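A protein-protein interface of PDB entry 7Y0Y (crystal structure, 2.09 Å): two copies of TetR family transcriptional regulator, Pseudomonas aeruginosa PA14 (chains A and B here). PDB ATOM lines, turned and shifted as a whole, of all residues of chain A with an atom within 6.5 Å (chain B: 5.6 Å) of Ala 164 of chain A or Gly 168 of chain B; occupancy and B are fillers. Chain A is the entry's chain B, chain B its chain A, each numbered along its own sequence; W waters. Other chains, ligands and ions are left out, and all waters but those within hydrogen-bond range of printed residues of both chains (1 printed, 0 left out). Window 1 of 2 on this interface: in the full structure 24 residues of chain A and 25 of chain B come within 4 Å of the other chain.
Of the 11 printed residues of chain B, 6 touch a printed residue of chain A.
Hydrophobic or aromatic side chains of chain B within 4 Å of the printed part of chain A: Trp 163, Ala 164, Ala 171 and Leu 172.
Printed residues of chain A that touch a printed residue of chain B: Cys 160, Trp 163, Ala 164, His 167, Gly 168 and Ala 169.
Hydrophobic or aromatic side chains of chain A within 4 Å of the printed part of chain B: Trp 163, Ala 164 and His 167.
Among the printed residues, no Asp or Glu carboxylate lies within 4 Å of a Lys or Arg side-chain nitrogen of the other chain.
Water W1 lies within hydrogen-bond range of NE2 of His 167 of chain B (2.9 Å) and NE2 of His 167 of chain A (3.0 Å).
Among the printed residues, merely in contact across the chains: His 167 of chain A with Ala 171 of chain B (3.2 Å), Ala 164 of chain A with Gly 168 of chain B (3.2 Å), Gly 168 of chain A with Ala 164 of chain B (3.2 Å), Cys 160 of chain A with Leu 172 of chain B (3.5 Å), Trp 163 of chain A with Leu 172 of chain B (3.6 Å), Gly 168 of chain A with Trp 163 of chain B (3.7 Å), Ala 169 of chain A with Ala 164 of chain B (3.7 Å), Ala 164 of chain A with Ala 169 of chain B (3.8 Å), Gly 168 of chain A with Gly 168 of chain B (3.8 Å), Trp 163 of chain A with Ala 171 of chain B (3.8 Å) and Trp 163 of chain A with Gly 168 of chain B (3.96 Å).
Trp 163 of chain A touches Gly 168 of chain B, and with the chains exchanged Gly 168 of chain A touches Trp 163 of chain B.
Ala 164 of chain A touches Gly 168 of chain B, and with the chains exchanged Gly 168 of chain A touches Ala 164 of chain B.
Ala 164 of chain A touches Ala 169 of chain B, and with the chains exchanged Ala 169 of chain A touches Ala 164 of chain B.
Gly 168 of chain A touches its own counterpart, Gly 168 of chain B.
Ala 164 of chain A touches just these residues of chain B: Gly 168 (3.2 Å) and Ala 169 (3.8 Å).
Of chain A, only Trp 163 (3.96 Å), Ala 164 (3.2 Å) and Gly 168 (3.8 Å) come within 4 Å of Gly 168 of chain B.
Of the printed residues of chain B, Cys 160 of chain A touches Leu 172.
Of the printed residues of chain A, Ala 169 of chain B touches Ala 164 (3.8 Å).
Of the printed residues of chain A, Trp 163 of chain B touches Gly 168 (3.7 Å).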
ATOM      1  N   TYR A 159     -25.510  22.965 -32.204  1.00  0.00           N
ATOM      2  CA  TYR A 159     -26.944  23.239 -32.169  1.00  0.00           C
ATOM      3  C   TYR A 159     -27.547  22.831 -30.833  1.00  0.00           C
ATOM      4  O   TYR A 159     -28.345  23.570 -30.253  1.00  0.00           O
ATOM      5  CB  TYR A 159     -27.671  22.517 -33.310  1.00  0.00           C
ATOM      6  CG  TYR A 159     -29.090  23.015 -33.488  1.00  0.00           C
ATOM      7  CD1 TYR A 159     -29.415  23.897 -34.513  1.00  0.00           C
ATOM      8  CD2 TYR A 159     -30.111  22.624 -32.616  1.00  0.00           C
ATOM      9  CE1 TYR A 159     -30.728  24.360 -34.682  1.00  0.00           C
ATOM     10  CE2 TYR A 159     -31.413  23.109 -32.759  1.00  0.00           C
ATOM     11  CZ  TYR A 159     -31.712  23.979 -33.794  1.00  0.00           C
ATOM     12  OH  TYR A 159     -33.000  24.453 -33.982  1.00  0.00           O
ATOM     13  N   CYS A 160     -27.194  21.638 -30.337  1.00  0.00           N
ATOM     14  CA  CYS A 160     -27.727  21.202 -29.050  1.00  0.00           C
ATOM     15  C   CYS A 160     -27.218  22.074 -27.907  1.00  0.00           C
ATOM     16  O   CYS A 160     -27.959  22.349 -26.963  1.00  0.00           O
ATOM     17  CB  CYS A 160     -27.381  19.738 -28.799  1.00  0.00           C
ATOM     18  SG  CYS A 160     -28.097  18.626 -30.029  1.00  0.00           S
ATOM     19  N   ALA A 161     -25.956  22.518 -27.970  1.00  0.00           N
ATOM     20  CA  ALA A 161     -25.433  23.405 -26.933  1.00  0.00           C
ATOM     21  C   ALA A 161     -26.204  24.721 -26.892  1.00  0.00           C
ATOM     22  O   ALA A 161     -26.431  25.288 -25.813  1.00  0.00           O
ATOM     23  CB  ALA A 161     -23.943  23.676 -27.177  1.00  0.00           C
ATOM     24  N   ALA A 162     -26.595  25.235 -28.065  1.00  0.00           N
ATOM     25  CA  ALA A 162     -27.362  26.478 -28.128  1.00  0.00           C
ATOM     26  C   ALA A 162     -28.780  26.279 -27.602  1.00  0.00           C
ATOM     27  O   ALA A 162     -29.291  27.123 -26.856  1.00  0.00           O
ATOM     28  CB  ALA A 162     -27.391  27.007 -29.565  1.00  0.00           C
ATOM     29  N   TRP A 163     -29.434  25.173 -27.986  1.00  0.00           N
ATOM     30  CA  TRP A 163     -30.728  24.838 -27.398  1.00  0.00           C
ATOM     31  C   TRP A 163     -30.656  24.769 -25.873  1.00  0.00           C
ATOM     32  O   TRP A 163     -31.553  25.253 -25.170  1.00  0.00           O
ATOM     33  CB  TRP A 163     -31.232  23.510 -27.959  1.00  0.00           C
ATOM     34  CG  TRP A 163     -32.667  23.246 -27.595  1.00  0.00           C
ATOM     35  CD1 TRP A 163     -33.770  23.580 -28.327  1.00  0.00           C
ATOM     36  CD2 TRP A 163     -33.154  22.625 -26.390  1.00  0.00           C
ATOM     37  NE1 TRP A 163     -34.909  23.197 -27.659  1.00  0.00           N
ATOM     38  CE2 TRP A 163     -34.561  22.603 -26.474  1.00  0.00           C
ATOM     39  CE3 TRP A 163     -32.540  22.070 -25.269  1.00  0.00           C
ATOM     40  CZ2 TRP A 163     -35.359  22.055 -25.471  1.00  0.00           C
ATOM     41  CZ3 TRP A 163     -33.337  21.520 -24.271  1.00  0.00           C
ATOM     42  CH2 TRP A 163     -34.729  21.523 -24.377  1.00  0.00           C
ATOM     43  N   ALA A 164     -29.596  24.162 -25.344  1.00  0.00           N
ATOM     44  CA  ALA A 164     -29.489  23.985 -23.899  1.00  0.00           C
ATOM     45  C   ALA A 164     -29.309  25.316 -23.184  1.00  0.00           C
ATOM     46  O   ALA A 164     -29.934  25.555 -22.146  1.00  0.00           O
ATOM     47  CB  ALA A 164     -28.335  23.035 -23.578  1.00  0.00           C
ATOM     48  N   LEU A 165     -28.447  26.190 -23.714  1.00  0.00           N
ATOM     49  CA  LEU A 165     -28.224  27.477 -23.077  1.00  0.00           C
ATOM     50  C   LEU A 165     -29.498  28.308 -23.061  1.00  0.00           C
ATOM     51  O   LEU A 165     -29.823  28.938 -22.048  1.00  0.00           O
ATOM     52  CB  LEU A 165     -27.109  28.242 -23.791  1.00  0.00           C
ATOM     53  CG  LEU A 165     -26.690  29.548 -23.111  1.00  0.00           C
ATOM     54  CD1 LEU A 165     -25.844  29.255 -21.872  1.00  0.00           C
ATOM     55  CD2 LEU A 165     -25.934  30.436 -24.081  1.00  0.00           C
ATOM     56  N   VAL A 166     -30.217  28.342 -24.182  1.00  0.00           N
ATOM     57  CA  VAL A 166     -31.469  29.078 -24.235  1.00  0.00           C
ATOM     58  C   VAL A 166     -32.468  28.480 -23.255  1.00  0.00           C
ATOM     59  O   VAL A 166     -33.090  29.197 -22.459  1.00  0.00           O
ATOM     60  CB  VAL A 166     -32.029  29.085 -25.669  1.00  0.00           C
ATOM     61  CG1 VAL A 166     -33.458  29.706 -25.662  1.00  0.00           C
ATOM     62  CG2 VAL A 166     -31.072  29.841 -26.591  1.00  0.00           C
ATOM     63  N   HIS A 167     -32.625  27.153 -23.286  1.00  0.00           N
ATOM     64  CA  HIS A 167     -33.602  26.515 -22.405  1.00  0.00           C
ATOM     65  C   HIS A 167     -33.264  26.752 -20.941  1.00  0.00           C
ATOM     66  O   HIS A 167     -34.151  27.045 -20.133  1.00  0.00           O
ATOM     67  CB  HIS A 167     -33.691  25.017 -22.680  1.00  0.00           C
ATOM     68  CG  HIS A 167     -34.856  24.359 -22.012  1.00  0.00           C
ATOM     69  ND1 HIS A 167     -36.148  24.476 -22.485  1.00  0.00           N
ATOM     70  CD2 HIS A 167     -34.933  23.615 -20.882  1.00  0.00           C
ATOM     71  CE1 HIS A 167     -36.964  23.806 -21.690  1.00  0.00           C
ATOM     72  NE2 HIS A 167     -36.252  23.272 -20.711  1.00  0.00           N
ATOM     73  N   GLY A 168     -31.988  26.623 -20.576  1.00  0.00           N
ATOM     74  CA  GLY A 168     -31.605  26.872 -19.199  1.00  0.00           C
ATOM     75  C   GLY A 168     -31.748  28.329 -18.819  1.00  0.00           C
ATOM     76  O   GLY A 168     -32.054  28.649 -17.665  1.00  0.00           O
ATOM     77  N   ALA A 169     -31.504  29.232 -19.774  1.00  0.00           N
ATOM     78  CA  ALA A 169     -31.687  30.656 -19.505  1.00  0.00           C
ATOM     79  C   ALA A 169     -33.152  30.979 -19.232  1.00  0.00           C
ATOM     80  O   ALA A 169     -33.461  31.759 -18.336  1.00  0.00           O
ATOM     81  CB  ALA A 169     -31.166  31.487 -20.687  1.00  0.00           C
ATOM     82  N   MET A 199     -19.506  30.147 -27.033  1.00  0.00           N
ATOM     83  CA  MET A 199     -19.304  28.763 -26.629  1.00  0.00           C
ATOM     84  C   MET A 199     -19.020  27.943 -27.876  1.00  0.00           C
ATOM     85  O   MET A 199     -19.457  28.271 -28.990  1.00  0.00           O
ATOM     86  CB  MET A 199     -20.464  28.184 -25.776  1.00  0.00           C
ATOM     87  CG  MET A 199     -21.805  28.092 -26.361  1.00  0.00           C
ATOM     88  SD  MET A 199     -23.200  27.298 -25.152  1.00  0.00           S
ATOM     89  CE  MET A 199     -24.563  27.813 -26.398  1.00  0.00           C
ATOM     90  N   TRP B 163     -25.673  27.757 -13.709  1.00  0.00           N
ATOM     91  CA  TRP B 163     -26.985  27.177 -13.422  1.00  0.00           C
ATOM     92  C   TRP B 163     -27.769  26.945 -14.708  1.00  0.00           C
ATOM     93  O   TRP B 163     -28.427  25.905 -14.875  1.00  0.00           O
ATOM     94  CB  TRP B 163     -27.762  28.097 -12.470  1.00  0.00           C
ATOM     95  CG  TRP B 163     -29.028  27.518 -11.903  1.00  0.00           C
ATOM     96  CD1 TRP B 163     -29.201  26.990 -10.646  1.00  0.00           C
ATOM     97  CD2 TRP B 163     -30.312  27.433 -12.554  1.00  0.00           C
ATOM     98  NE1 TRP B 163     -30.503  26.561 -10.492  1.00  0.00           N
ATOM     99  CE2 TRP B 163     -31.203  26.813 -11.646  1.00  0.00           C
ATOM    100  CE3 TRP B 163     -30.784  27.791 -13.824  1.00  0.00           C
ATOM    101  CZ2 TRP B 163     -32.549  26.555 -11.966  1.00  0.00           C
ATOM    102  CZ3 TRP B 163     -32.131  27.520 -14.142  1.00  0.00           C
ATOM    103  CH2 TRP B 163     -32.986  26.919 -13.215  1.00  0.00           C
ATOM    104  N   ALA B 164     -27.720  27.908 -15.627  1.00  0.00           N
ATOM    105  CA  ALA B 164     -28.464  27.769 -16.871  1.00  0.00           C
ATOM    106  C   ALA B 164     -27.910  26.635 -17.729  1.00  0.00           C
ATOM    107  O   ALA B 164     -28.674  25.841 -18.298  1.00  0.00           O
ATOM    108  CB  ALA B 164     -28.442  29.094 -17.633  1.00  0.00           C
ATOM    109  N   LEU B 165     -26.587  26.528 -17.838  1.00  0.00           N
ATOM    110  CA  LEU B 165     -26.038  25.495 -18.714  1.00  0.00           C
ATOM    111  C   LEU B 165     -26.408  24.103 -18.209  1.00  0.00           C
ATOM    112  O   LEU B 165     -26.868  23.254 -18.982  1.00  0.00           O
ATOM    113  CB  LEU B 165     -24.516  25.643 -18.838  1.00  0.00           C
ATOM    114  CG  LEU B 165     -23.866  24.659 -19.829  1.00  0.00           C
ATOM    115  CD1 LEU B 165     -24.179  25.037 -21.281  1.00  0.00           C
ATOM    116  CD2 LEU B 165     -22.375  24.602 -19.618  1.00  0.00           C
ATOM    117  N   VAL B 166     -26.219  23.862 -16.913  1.00  0.00           N
ATOM    118  CA  VAL B 166     -26.587  22.577 -16.324  1.00  0.00           C
ATOM    119  C   VAL B 166     -28.056  22.285 -16.576  1.00  0.00           C
ATOM    120  O   VAL B 166     -28.416  21.212 -17.073  1.00  0.00           O
ATOM    121  CB  VAL B 166     -26.270  22.563 -14.816  1.00  0.00           C
ATOM    122  CG1 VAL B 166     -26.797  21.272 -14.170  1.00  0.00           C
ATOM    123  CG2 VAL B 166     -24.774  22.708 -14.576  1.00  0.00           C
ATOM    124  N   HIS B 167     -28.929  23.247 -16.247  1.00  0.00           N
ATOM    125  CA  HIS B 167     -30.365  23.013 -16.376  1.00  0.00           C
ATOM    126  C   HIS B 167     -30.755  22.652 -17.799  1.00  0.00           C
ATOM    127  O   HIS B 167     -31.586  21.757 -18.016  1.00  0.00           O
ATOM    128  CB  HIS B 167     -31.155  24.235 -15.916  1.00  0.00           C
ATOM    129  CG  HIS B 167     -32.629  23.975 -15.829  1.00  0.00           C
ATOM    130  ND1 HIS B 167     -33.232  23.533 -14.674  1.00  0.00           N
ATOM    131  CD2 HIS B 167     -33.603  24.023 -16.768  1.00  0.00           C
ATOM    132  CE1 HIS B 167     -34.525  23.363 -14.893  1.00  0.00           C
ATOM    133  NE2 HIS B 167     -34.774  23.643 -16.159  1.00  0.00           N
ATOM    134  N   GLY B 168     -30.205  23.366 -18.788  1.00  0.00           N
ATOM    135  CA  GLY B 168     -30.553  23.077 -20.162  1.00  0.00           C
ATOM    136  C   GLY B 168     -29.944  21.788 -20.671  1.00  0.00           C
ATOM    137  O   GLY B 168     -30.553  21.089 -21.487  1.00  0.00           O
ATOM    138  N   ALA B 169     -28.744  21.441 -20.194  1.00  0.00           N
ATOM    139  CA  ALA B 169     -28.136  20.176 -20.609  1.00  0.00           C
ATOM    140  C   ALA B 169     -28.961  18.989 -20.125  1.00  0.00           C
ATOM    141  O   ALA B 169     -29.152  18.013 -20.856  1.00  0.00           O
ATOM    142  CB  ALA B 169     -26.710  20.090 -20.080  1.00  0.00           C
ATOM    143  N   VAL B 170     -29.480  19.072 -18.896  1.00  0.00           N
ATOM    144  CA  VAL B 170     -30.385  18.042 -18.391  1.00  0.00           C
ATOM    145  C   VAL B 170     -31.654  17.982 -19.234  1.00  0.00           C
ATOM    146  O   VAL B 170     -32.129  16.901 -19.595  1.00  0.00           O
ATOM    147  CB  VAL B 170     -30.707  18.303 -16.909  1.00  0.00           C
ATOM    148  CG1 VAL B 170     -31.768  17.329 -16.425  1.00  0.00           C
ATOM    149  CG2 VAL B 170     -29.458  18.221 -16.089  1.00  0.00           C
ATOM    150  N   ALA B 171     -32.230  19.145 -19.543  1.00  0.00           N
ATOM    151  CA  ALA B 171     -33.401  19.186 -20.408  1.00  0.00           C
ATOM    152  C   ALA B 171     -33.106  18.577 -21.770  1.00  0.00           C
ATOM    153  O   ALA B 171     -33.946  17.874 -22.341  1.00  0.00           O
ATOM    154  CB  ALA B 171     -33.874  20.625 -20.571  1.00  0.00           C
ATOM    155  N   LEU B 172     -31.923  18.860 -22.315  1.00  0.00           N
ATOM    156  CA  LEU B 172     -31.518  18.275 -23.589  1.00  0.00           C
ATOM    157  C   LEU B 172     -31.599  16.760 -23.531  1.00  0.00           C
ATOM    158  O   LEU B 172     -32.228  16.122 -24.381  1.00  0.00           O
ATOM    159  CB  LEU B 172     -30.094  18.731 -23.914  1.00  0.00           C
ATOM    160  CG  LEU B 172     -29.526  18.663 -25.318  1.00  0.00           C
ATOM    161  CD1 LEU B 172     -30.422  19.379 -26.289  1.00  0.00           C
ATOM    162  CD2 LEU B 172     -28.151  19.318 -25.276  1.00  0.00           C
ATOM    163  N   TYR B 173     -30.999  16.175 -22.497  1.00  0.00           N
ATOM    164  CA  TYR B 173     -30.946  14.728 -22.361  1.00  0.00           C
ATOM    165  C   TYR B 173     -32.324  14.113 -22.182  1.00  0.00           C
ATOM    166  O   TYR B 173     -32.475  12.907 -22.385  1.00  0.00           O
ATOM    167  CB  TYR B 173     -30.042  14.347 -21.178  1.00  0.00           C
ATOM    168  CG  TYR B 173     -28.547  14.526 -21.447  1.00  0.00           C
ATOM    169  CD1 TYR B 173     -27.921  13.857 -22.506  1.00  0.00           C
ATOM    170  CD2 TYR B 173     -27.760  15.341 -20.630  1.00  0.00           C
ATOM    171  CE1 TYR B 173     -26.557  14.016 -22.757  1.00  0.00           C
ATOM    172  CE2 TYR B 173     -26.399  15.506 -20.869  1.00  0.00           C
ATOM    173  CZ  TYR B 173     -25.802  14.837 -21.935  1.00  0.00           C
ATOM    174  OH  TYR B 173     -24.452  14.983 -22.177  1.00  0.00           O
HETATM  175  O   HOH W   1     -37.095  24.039 -17.906  1.00  0.00           O
